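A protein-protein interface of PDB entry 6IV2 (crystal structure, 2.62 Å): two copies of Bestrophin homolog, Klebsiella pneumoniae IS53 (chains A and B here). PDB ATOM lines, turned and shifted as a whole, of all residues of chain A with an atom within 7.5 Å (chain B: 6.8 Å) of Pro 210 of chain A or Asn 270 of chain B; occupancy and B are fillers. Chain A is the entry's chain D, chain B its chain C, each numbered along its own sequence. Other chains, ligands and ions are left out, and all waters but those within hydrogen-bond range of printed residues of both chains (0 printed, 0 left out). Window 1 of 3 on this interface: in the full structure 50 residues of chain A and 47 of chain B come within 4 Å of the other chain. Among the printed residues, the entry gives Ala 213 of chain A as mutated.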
ATOM      1  N   ARG A  73     -16.210 -16.751   5.610  1.00  0.00           N
ATOM      2  CA  ARG A  73     -15.315 -15.807   6.263  1.00  0.00           C
ATOM      3  C   ARG A  73     -13.861 -16.117   5.924  1.00  0.00           C
ATOM      4  O   ARG A  73     -13.102 -15.227   5.527  1.00  0.00           O
ATOM      5  CB  ARG A  73     -15.550 -15.839   7.774  1.00  0.00           C
ATOM      6  CG  ARG A  73     -14.993 -14.659   8.522  1.00  0.00           C
ATOM      7  CD  ARG A  73     -13.562 -14.922   8.891  1.00  0.00           C
ATOM      8  NE  ARG A  73     -13.423 -16.163   9.634  1.00  0.00           N
ATOM      9  CZ  ARG A  73     -13.567 -16.259  10.949  1.00  0.00           C
ATOM     10  NH1 ARG A  73     -13.858 -15.181  11.661  1.00  0.00           N
ATOM     11  NH2 ARG A  73     -13.410 -17.430  11.554  1.00  0.00           N
ATOM     12  N   ALA A  76     -12.810 -14.932   2.620  1.00  0.00           N
ATOM     13  CA  ALA A  76     -12.500 -13.508   2.660  1.00  0.00           C
ATOM     14  C   ALA A  76     -11.136 -13.266   3.291  1.00  0.00           C
ATOM     15  O   ALA A  76     -10.297 -12.554   2.729  1.00  0.00           O
ATOM     16  CB  ALA A  76     -13.585 -12.756   3.428  1.00  0.00           C
ATOM     17  N   SER A  77     -10.889 -13.873   4.459  1.00  0.00           N
ATOM     18  CA  SER A  77      -9.611 -13.690   5.137  1.00  0.00           C
ATOM     19  C   SER A  77      -8.450 -14.153   4.273  1.00  0.00           C
ATOM     20  O   SER A  77      -7.375 -13.542   4.293  1.00  0.00           O
ATOM     21  CB  SER A  77      -9.606 -14.436   6.468  1.00  0.00           C
ATOM     22  OG  SER A  77     -10.644 -13.980   7.307  1.00  0.00           O
ATOM     23  N   THR A 207      -8.222  -1.866   7.182  1.00  0.00           N
ATOM     24  CA  THR A 207      -9.539  -2.446   6.917  1.00  0.00           C
ATOM     25  C   THR A 207      -9.515  -3.940   7.215  1.00  0.00           C
ATOM     26  O   THR A 207      -9.241  -4.757   6.321  1.00  0.00           O
ATOM     27  CB  THR A 207      -9.973  -2.186   5.473  1.00  0.00           C
ATOM     28  OG1 THR A 207      -9.625  -0.846   5.100  1.00  0.00           O
ATOM     29  CG2 THR A 207     -11.480  -2.370   5.322  1.00  0.00           C
ATOM     30  N   PRO A 208      -9.808  -4.344   8.449  1.00  0.00           N
ATOM     31  CA  PRO A 208      -9.883  -5.776   8.756  1.00  0.00           C
ATOM     32  C   PRO A 208     -11.149  -6.397   8.185  1.00  0.00           C
ATOM     33  O   PRO A 208     -12.145  -5.717   7.921  1.00  0.00           O
ATOM     34  CB  PRO A 208      -9.894  -5.810  10.287  1.00  0.00           C
ATOM     35  CG  PRO A 208     -10.544  -4.506  10.672  1.00  0.00           C
ATOM     36  CD  PRO A 208     -10.114  -3.502   9.622  1.00  0.00           C
ATOM     37  N   VAL A 209     -11.093  -7.709   7.973  1.00  0.00           N
ATOM     38  CA  VAL A 209     -12.301  -8.474   7.671  1.00  0.00           C
ATOM     39  C   VAL A 209     -13.228  -8.215   8.852  1.00  0.00           C
ATOM     40  O   VAL A 209     -12.808  -8.395  10.006  1.00  0.00           O
ATOM     41  CB  VAL A 209     -12.005  -9.971   7.469  1.00  0.00           C
ATOM     42  CG1 VAL A 209     -13.294 -10.802   7.533  1.00  0.00           C
ATOM     43  CG2 VAL A 209     -11.298 -10.201   6.143  1.00  0.00           C
ATOM     44  N   PRO A 210     -14.484  -7.774   8.609  1.00  0.00           N
ATOM     45  CA  PRO A 210     -15.308  -7.158   9.663  1.00  0.00           C
ATOM     46  C   PRO A 210     -15.200  -7.758  11.057  1.00  0.00           C
ATOM     47  O   PRO A 210     -15.206  -8.982  11.233  1.00  0.00           O
ATOM     48  CB  PRO A 210     -16.729  -7.326   9.109  1.00  0.00           C
ATOM     49  CG  PRO A 210     -16.547  -7.197   7.634  1.00  0.00           C
ATOM     50  CD  PRO A 210     -15.190  -7.805   7.315  1.00  0.00           C
ATOM     51  N   PHE A 211     -15.075  -6.874  12.050  1.00  0.00           N
ATOM     52  CA  PHE A 211     -15.117  -7.295  13.444  1.00  0.00           C
ATOM     53  C   PHE A 211     -16.337  -8.168  13.707  1.00  0.00           C
ATOM     54  O   PHE A 211     -16.238  -9.200  14.376  1.00  0.00           O
ATOM     55  CB  PHE A 211     -15.122  -6.064  14.353  1.00  0.00           C
ATOM     56  CG  PHE A 211     -14.782  -6.357  15.789  1.00  0.00           C
ATOM     57  CD1 PHE A 211     -13.714  -7.181  16.109  1.00  0.00           C
ATOM     58  CD2 PHE A 211     -15.520  -5.791  16.819  1.00  0.00           C
ATOM     59  CE1 PHE A 211     -13.394  -7.447  17.428  1.00  0.00           C
ATOM     60  CE2 PHE A 211     -15.203  -6.050  18.142  1.00  0.00           C
ATOM     61  CZ  PHE A 211     -14.139  -6.882  18.445  1.00  0.00           C
ATOM     62  N   ALA A 212     -17.491  -7.777  13.158  1.00  0.00           N
ATOM     63  CA  ALA A 212     -18.715  -8.546  13.357  1.00  0.00           C
ATOM     64  C   ALA A 212     -18.553  -9.982  12.871  1.00  0.00           C
ATOM     65  O   ALA A 212     -18.907 -10.930  13.579  1.00  0.00           O
ATOM     66  CB  ALA A 212     -19.880  -7.861  12.645  1.00  0.00           C
ATOM     67  N   ALA A 213     -18.015 -10.157  11.660  1.00  0.00           N
ATOM     68  CA  ALA A 213     -17.789 -11.490  11.117  1.00  0.00           C
ATOM     69  C   ALA A 213     -17.012 -12.352  12.102  1.00  0.00           C
ATOM     70  O   ALA A 213     -17.478 -13.415  12.527  1.00  0.00           O
ATOM     71  CB  ALA A 213     -17.046 -11.393   9.783  1.00  0.00           C
ATOM     72  N   THR A 214     -15.829 -11.882  12.499  1.00  0.00           N
ATOM     73  CA  THR A 214     -14.970 -12.683  13.361  1.00  0.00           C
ATOM     74  C   THR A 214     -15.526 -12.779  14.775  1.00  0.00           C
ATOM     75  O   THR A 214     -15.426 -13.835  15.410  1.00  0.00           O
ATOM     76  CB  THR A 214     -13.558 -12.104  13.365  1.00  0.00           C
ATOM     77  OG1 THR A 214     -13.145 -11.865  12.014  1.00  0.00           O
ATOM     78  CG2 THR A 214     -12.588 -13.071  14.024  1.00  0.00           C
ATOM     79  N   LEU A 215     -16.121 -11.693  15.279  1.00  0.00           N
ATOM     80  CA  LEU A 215     -16.718 -11.693  16.612  1.00  0.00           C
ATOM     81  C   LEU A 215     -17.830 -12.728  16.718  1.00  0.00           C
ATOM     82  O   LEU A 215     -17.822 -13.578  17.615  1.00  0.00           O
ATOM     83  CB  LEU A 215     -17.256 -10.296  16.937  1.00  0.00           C
ATOM     84  CG  LEU A 215     -17.636  -9.893  18.361  1.00  0.00           C
ATOM     85  CD1 LEU A 215     -17.716  -8.381  18.454  1.00  0.00           C
ATOM     86  CD2 LEU A 215     -18.969 -10.497  18.742  1.00  0.00           C
ATOM     87  N   ILE A 216     -18.829 -12.624  15.843  1.00  0.00           N
ATOM     88  CA  ILE A 216     -19.899 -13.610  15.741  1.00  0.00           C
ATOM     89  C   ILE A 216     -19.290 -14.999  15.718  1.00  0.00           C
ATOM     90  O   ILE A 216     -19.588 -15.841  16.572  1.00  0.00           O
ATOM     91  CB  ILE A 216     -20.755 -13.393  14.480  1.00  0.00           C
ATOM     92  CG1 ILE A 216     -21.659 -12.164  14.635  1.00  0.00           C
ATOM     93  CG2 ILE A 216     -21.545 -14.665  14.151  1.00  0.00           C
ATOM     94  CD1 ILE A 216     -22.004 -11.500  13.315  1.00  0.00           C
ATOM     95  N   GLU A 262      -5.174 -12.692   9.288  1.00  0.00           N
ATOM     96  CA  GLU A 262      -5.690 -11.356   9.548  1.00  0.00           C
ATOM     97  C   GLU A 262      -4.587 -10.317   9.665  1.00  0.00           C
ATOM     98  O   GLU A 262      -4.848  -9.128   9.459  1.00  0.00           O
ATOM     99  CB  GLU A 262      -6.529 -11.359  10.834  1.00  0.00           C
ATOM    100  CG  GLU A 262      -7.754 -10.446  10.799  1.00  0.00           C
ATOM    101  CD  GLU A 262      -9.032 -11.163  10.378  1.00  0.00           C
ATOM    102  OE1 GLU A 262      -9.672 -11.797  11.246  1.00  0.00           O
ATOM    103  OE2 GLU A 262      -9.406 -11.085   9.186  1.00  0.00           O
ATOM    104  N   TYR B  78     -20.659  -8.728   1.013  1.00  0.00           N
ATOM    105  CA  TYR B  78     -19.273  -8.376   1.309  1.00  0.00           C
ATOM    106  C   TYR B  78     -18.557  -7.845   0.069  1.00  0.00           C
ATOM    107  O   TYR B  78     -17.760  -6.903   0.158  1.00  0.00           O
ATOM    108  CB  TYR B  78     -18.542  -9.595   1.877  1.00  0.00           C
ATOM    109  CG  TYR B  78     -17.116  -9.324   2.300  1.00  0.00           C
ATOM    110  CD1 TYR B  78     -16.824  -8.347   3.242  1.00  0.00           C
ATOM    111  CD2 TYR B  78     -16.061 -10.052   1.764  1.00  0.00           C
ATOM    112  CE1 TYR B  78     -15.525  -8.100   3.636  1.00  0.00           C
ATOM    113  CE2 TYR B  78     -14.757  -9.806   2.147  1.00  0.00           C
ATOM    114  CZ  TYR B  78     -14.494  -8.833   3.086  1.00  0.00           C
ATOM    115  OH  TYR B  78     -13.197  -8.584   3.479  1.00  0.00           O
ATOM    116  N   PHE B  81     -19.313  -4.300  -0.537  1.00  0.00           N
ATOM    117  CA  PHE B  81     -18.581  -3.514   0.450  1.00  0.00           C
ATOM    118  C   PHE B  81     -17.098  -3.437   0.108  1.00  0.00           C
ATOM    119  O   PHE B  81     -16.489  -2.363   0.183  1.00  0.00           O
ATOM    120  CB  PHE B  81     -18.785  -4.113   1.838  1.00  0.00           C
ATOM    121  CG  PHE B  81     -17.997  -3.431   2.910  1.00  0.00           C
ATOM    122  CD1 PHE B  81     -18.530  -2.351   3.594  1.00  0.00           C
ATOM    123  CD2 PHE B  81     -16.725  -3.875   3.246  1.00  0.00           C
ATOM    124  CE1 PHE B  81     -17.809  -1.726   4.582  1.00  0.00           C
ATOM    125  CE2 PHE B  81     -15.996  -3.249   4.233  1.00  0.00           C
ATOM    126  CZ  PHE B  81     -16.539  -2.175   4.903  1.00  0.00           C
ATOM    127  N   LEU B 257     -25.553  -8.738   9.361  1.00  0.00           N
ATOM    128  CA  LEU B 257     -24.266  -8.281   8.856  1.00  0.00           C
ATOM    129  C   LEU B 257     -24.314  -8.100   7.346  1.00  0.00           C
ATOM    130  O   LEU B 257     -23.610  -7.248   6.793  1.00  0.00           O
ATOM    131  CB  LEU B 257     -23.171  -9.270   9.258  1.00  0.00           C
ATOM    132  CG  LEU B 257     -21.812  -9.163   8.575  1.00  0.00           C
ATOM    133  CD1 LEU B 257     -21.018  -8.006   9.162  1.00  0.00           C
ATOM    134  CD2 LEU B 257     -21.062 -10.478   8.717  1.00  0.00           C
ATOM    135  N   GLU B 260     -26.000  -4.546   6.578  1.00  0.00           N
ATOM    136  CA  GLU B 260     -25.146  -3.379   6.745  1.00  0.00           C
ATOM    137  C   GLU B 260     -23.972  -3.384   5.768  1.00  0.00           C
ATOM    138  O   GLU B 260     -23.529  -2.315   5.337  1.00  0.00           O
ATOM    139  CB  GLU B 260     -24.662  -3.285   8.193  1.00  0.00           C
ATOM    140  CG  GLU B 260     -23.770  -4.415   8.658  1.00  0.00           C
ATOM    141  CD  GLU B 260     -23.447  -4.308  10.133  1.00  0.00           C
ATOM    142  OE1 GLU B 260     -22.265  -4.456  10.496  1.00  0.00           O
ATOM    143  OE2 GLU B 260     -24.377  -4.072  10.933  1.00  0.00           O
ATOM    144  N   LEU B 261     -23.467  -4.561   5.388  1.00  0.00           N
ATOM    145  CA  LEU B 261     -22.483  -4.612   4.312  1.00  0.00           C
ATOM    146  C   LEU B 261     -23.103  -4.257   2.968  1.00  0.00           C
ATOM    147  O   LEU B 261     -22.377  -3.913   2.026  1.00  0.00           O
ATOM    148  CB  LEU B 261     -21.848  -6.003   4.244  1.00  0.00           C
ATOM    149  CG  LEU B 261     -20.839  -6.392   5.328  1.00  0.00           C
ATOM    150  CD1 LEU B 261     -20.381  -7.829   5.132  1.00  0.00           C
ATOM    151  CD2 LEU B 261     -19.651  -5.438   5.327  1.00  0.00           C
ATOM    152  N   ASP B 263     -25.168  -1.716   2.346  1.00  0.00           N
ATOM    153  CA  ASP B 263     -25.224  -0.268   2.251  1.00  0.00           C
ATOM    154  C   ASP B 263     -23.869   0.294   2.666  1.00  0.00           C
ATOM    155  O   ASP B 263     -23.746   0.875   3.751  1.00  0.00           O
ATOM    156  CB  ASP B 263     -26.353   0.255   3.145  1.00  0.00           C
ATOM    157  CG  ASP B 263     -26.496   1.761   3.107  1.00  0.00           C
ATOM    158  OD1 ASP B 263     -26.092   2.381   2.100  1.00  0.00           O
ATOM    159  OD2 ASP B 263     -27.021   2.322   4.095  1.00  0.00           O
ATOM    160  N   PRO B 264     -22.827   0.142   1.840  1.00  0.00           N
ATOM    161  CA  PRO B 264     -21.471   0.456   2.315  1.00  0.00           C
ATOM    162  C   PRO B 264     -21.216   1.938   2.520  1.00  0.00           C
ATOM    163  O   PRO B 264     -20.279   2.287   3.247  1.00  0.00           O
ATOM    164  CB  PRO B 264     -20.573  -0.124   1.216  1.00  0.00           C
ATOM    165  CG  PRO B 264     -21.405  -0.062  -0.003  1.00  0.00           C
ATOM    166  CD  PRO B 264     -22.833  -0.253   0.421  1.00  0.00           C
ATOM    167  N   THR B 267     -24.337   4.862   7.354  1.00  0.00           N
ATOM    168  CA  THR B 267     -23.796   5.356   8.615  1.00  0.00           C
ATOM    169  C   THR B 267     -23.753   4.284   9.699  1.00  0.00           C
ATOM    170  O   THR B 267     -23.510   4.609  10.866  1.00  0.00           O
ATOM    171  CB  THR B 267     -24.605   6.559   9.105  1.00  0.00           C
ATOM    172  OG1 THR B 267     -26.004   6.260   9.027  1.00  0.00           O
ATOM    173  CG2 THR B 267     -24.312   7.781   8.248  1.00  0.00           C
ATOM    174  N   ALA B 268     -23.963   3.020   9.343  1.00  0.00           N
ATOM    175  CA  ALA B 268     -24.007   1.939  10.319  1.00  0.00           C
ATOM    176  C   ALA B 268     -22.623   1.725  10.936  1.00  0.00           C
ATOM    177  O   ALA B 268     -21.673   2.480  10.703  1.00  0.00           O
ATOM    178  CB  ALA B 268     -24.540   0.663   9.672  1.00  0.00           C
ATOM    179  N   ALA B 269     -22.502   0.669  11.742  1.00  0.00           N
ATOM    180  CA  ALA B 269     -21.256   0.412  12.454  1.00  0.00           C
ATOM    181  C   ALA B 269     -20.150   0.009  11.488  1.00  0.00           C
ATOM    182  O   ALA B 269     -19.091   0.646  11.434  1.00  0.00           O
ATOM    183  CB  ALA B 269     -21.472  -0.667  13.517  1.00  0.00           C
ATOM    184  N   ASN B 270     -20.378  -1.051  10.712  1.00  0.00           N
ATOM    185  CA  ASN B 270     -19.397  -1.537   9.752  1.00  0.00           C
ATOM    186  C   ASN B 270     -19.556  -0.895   8.377  1.00  0.00           C
ATOM    187  O   ASN B 270     -19.116  -1.472   7.376  1.00  0.00           O
ATOM    188  CB  ASN B 270     -19.471  -3.064   9.651  1.00  0.00           C
ATOM    189  CG  ASN B 270     -19.488  -3.738  11.016  1.00  0.00           C
ATOM    190  OD1 ASN B 270     -20.224  -3.324  11.911  1.00  0.00           O
ATOM    191  ND2 ASN B 270     -18.677  -4.779  11.179  1.00  0.00           N
ATOM    192  N   ASP B 271     -20.165   0.286   8.311  1.00  0.00           N
ATOM    193  CA  ASP B 271     -20.187   1.062   7.085  1.00  0.00           C
ATOM    194  C   ASP B 271     -18.917   1.898   6.964  1.00  0.00           C
ATOM    195  O   ASP B 271     -18.180   2.103   7.932  1.00  0.00           O
ATOM    196  CB  ASP B 271     -21.420   1.961   7.032  1.00  0.00           C
ATOM    197  CG  ASP B 271     -22.662   1.210   6.599  1.00  0.00           C
ATOM    198  OD1 ASP B 271     -22.519   0.093   6.058  1.00  0.00           O
ATOM    199  OD2 ASP B 271     -23.775   1.732   6.798  1.00  0.00           O
ATOM    200  N   LEU B 272     -18.671   2.384   5.759  1.00  0.00           N
ATOM    201  CA  LEU B 272     -17.395   3.024   5.466  1.00  0.00           C
ATOM    202  C   LEU B 272     -17.269   4.342   6.224  1.00  0.00           C
ATOM    203  O   LEU B 272     -18.190   5.167   6.185  1.00  0.00           O
ATOM    204  CB  LEU B 272     -17.251   3.254   3.961  1.00  0.00           C
ATOM    205  CG  LEU B 272     -16.995   1.998   3.123  1.00  0.00           C
ATOM    206  CD1 LEU B 272     -16.856   2.350   1.657  1.00  0.00           C
ATOM    207  CD2 LEU B 272     -15.742   1.294   3.616  1.00  0.00           C
ATOM    208  N   PRO B 273     -16.152   4.579   6.917  1.00  0.00           N
ATOM    209  CA  PRO B 273     -15.946   5.872   7.579  1.00  0.00           C
ATOM    210  C   PRO B 273     -15.600   6.979   6.593  1.00  0.00           C
ATOM    211  O   PRO B 273     -14.468   7.466   6.582  1.00  0.00           O
ATOM    212  CB  PRO B 273     -14.770   5.580   8.517  1.00  0.00           C
ATOM    213  CG  PRO B 273     -13.964   4.592   7.746  1.00  0.00           C
ATOM    214  CD  PRO B 273     -14.973   3.705   7.052  1.00  0.00           C
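The side-chain carboxylate of Glu 260 of chain B sits close to the side-chain amide oxygen of Asn 270 of chain B, at 2.7 Å.
Among the printed residues, pairs that only touch across the chains: Ala 76 of chain A with Tyr 78 of chain B, Val 209 of chain A with Tyr 78 of chain B, Pro 210 of chain A with Tyr 78 of chain B, Pro 210 of chain A with Asn 270 of chain B, Ala 212 of chain A with Leu 257 of chain B and Ala 212 of chain A with Asn 270 of chain B.
Printed residues of chain B within 4 Å of Ala 76 of chain A: Tyr 78. Of the printed residues of chain B, Val 209 of chain A touches Tyr 78 (3.6 Å). Of the printed residues of chain A, Tyr 78 of chain B touches Ala 76 (3.4 Å), Val 209 (3.6 Å) and Pro 210 (3.7 Å). Of the printed residues of chain A, Leu 257 of chain B touches Ala 212 (3.7 Å). Thr 267 of chain B touches none of the printed residues of chain A. No residue of chain A comes within 4 Å of Ala 269 of chain B. The nearest printed residue of chain A that does not touch Tyr 78 of chain B is Pro 208 of chain A (5.4 Å).
Hydrophobic or aromatic side chains of chain B that line the printed part of chain A: Tyr 78 and Leu 257. Of the 14 printed residues of chain A, 4 touch a printed residue of chain B. Among the printed residues, 6 pairs touch across the chains. Among the printed residues, no Asp or Glu carboxylate lies within 4 Å of a Lys or Arg side-chain nitrogen of the other chain.
No position is printed for both chains. Of the 6 pairs that touch across the chains among the printed residues, none has its exchanged pair printed and touching as well.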
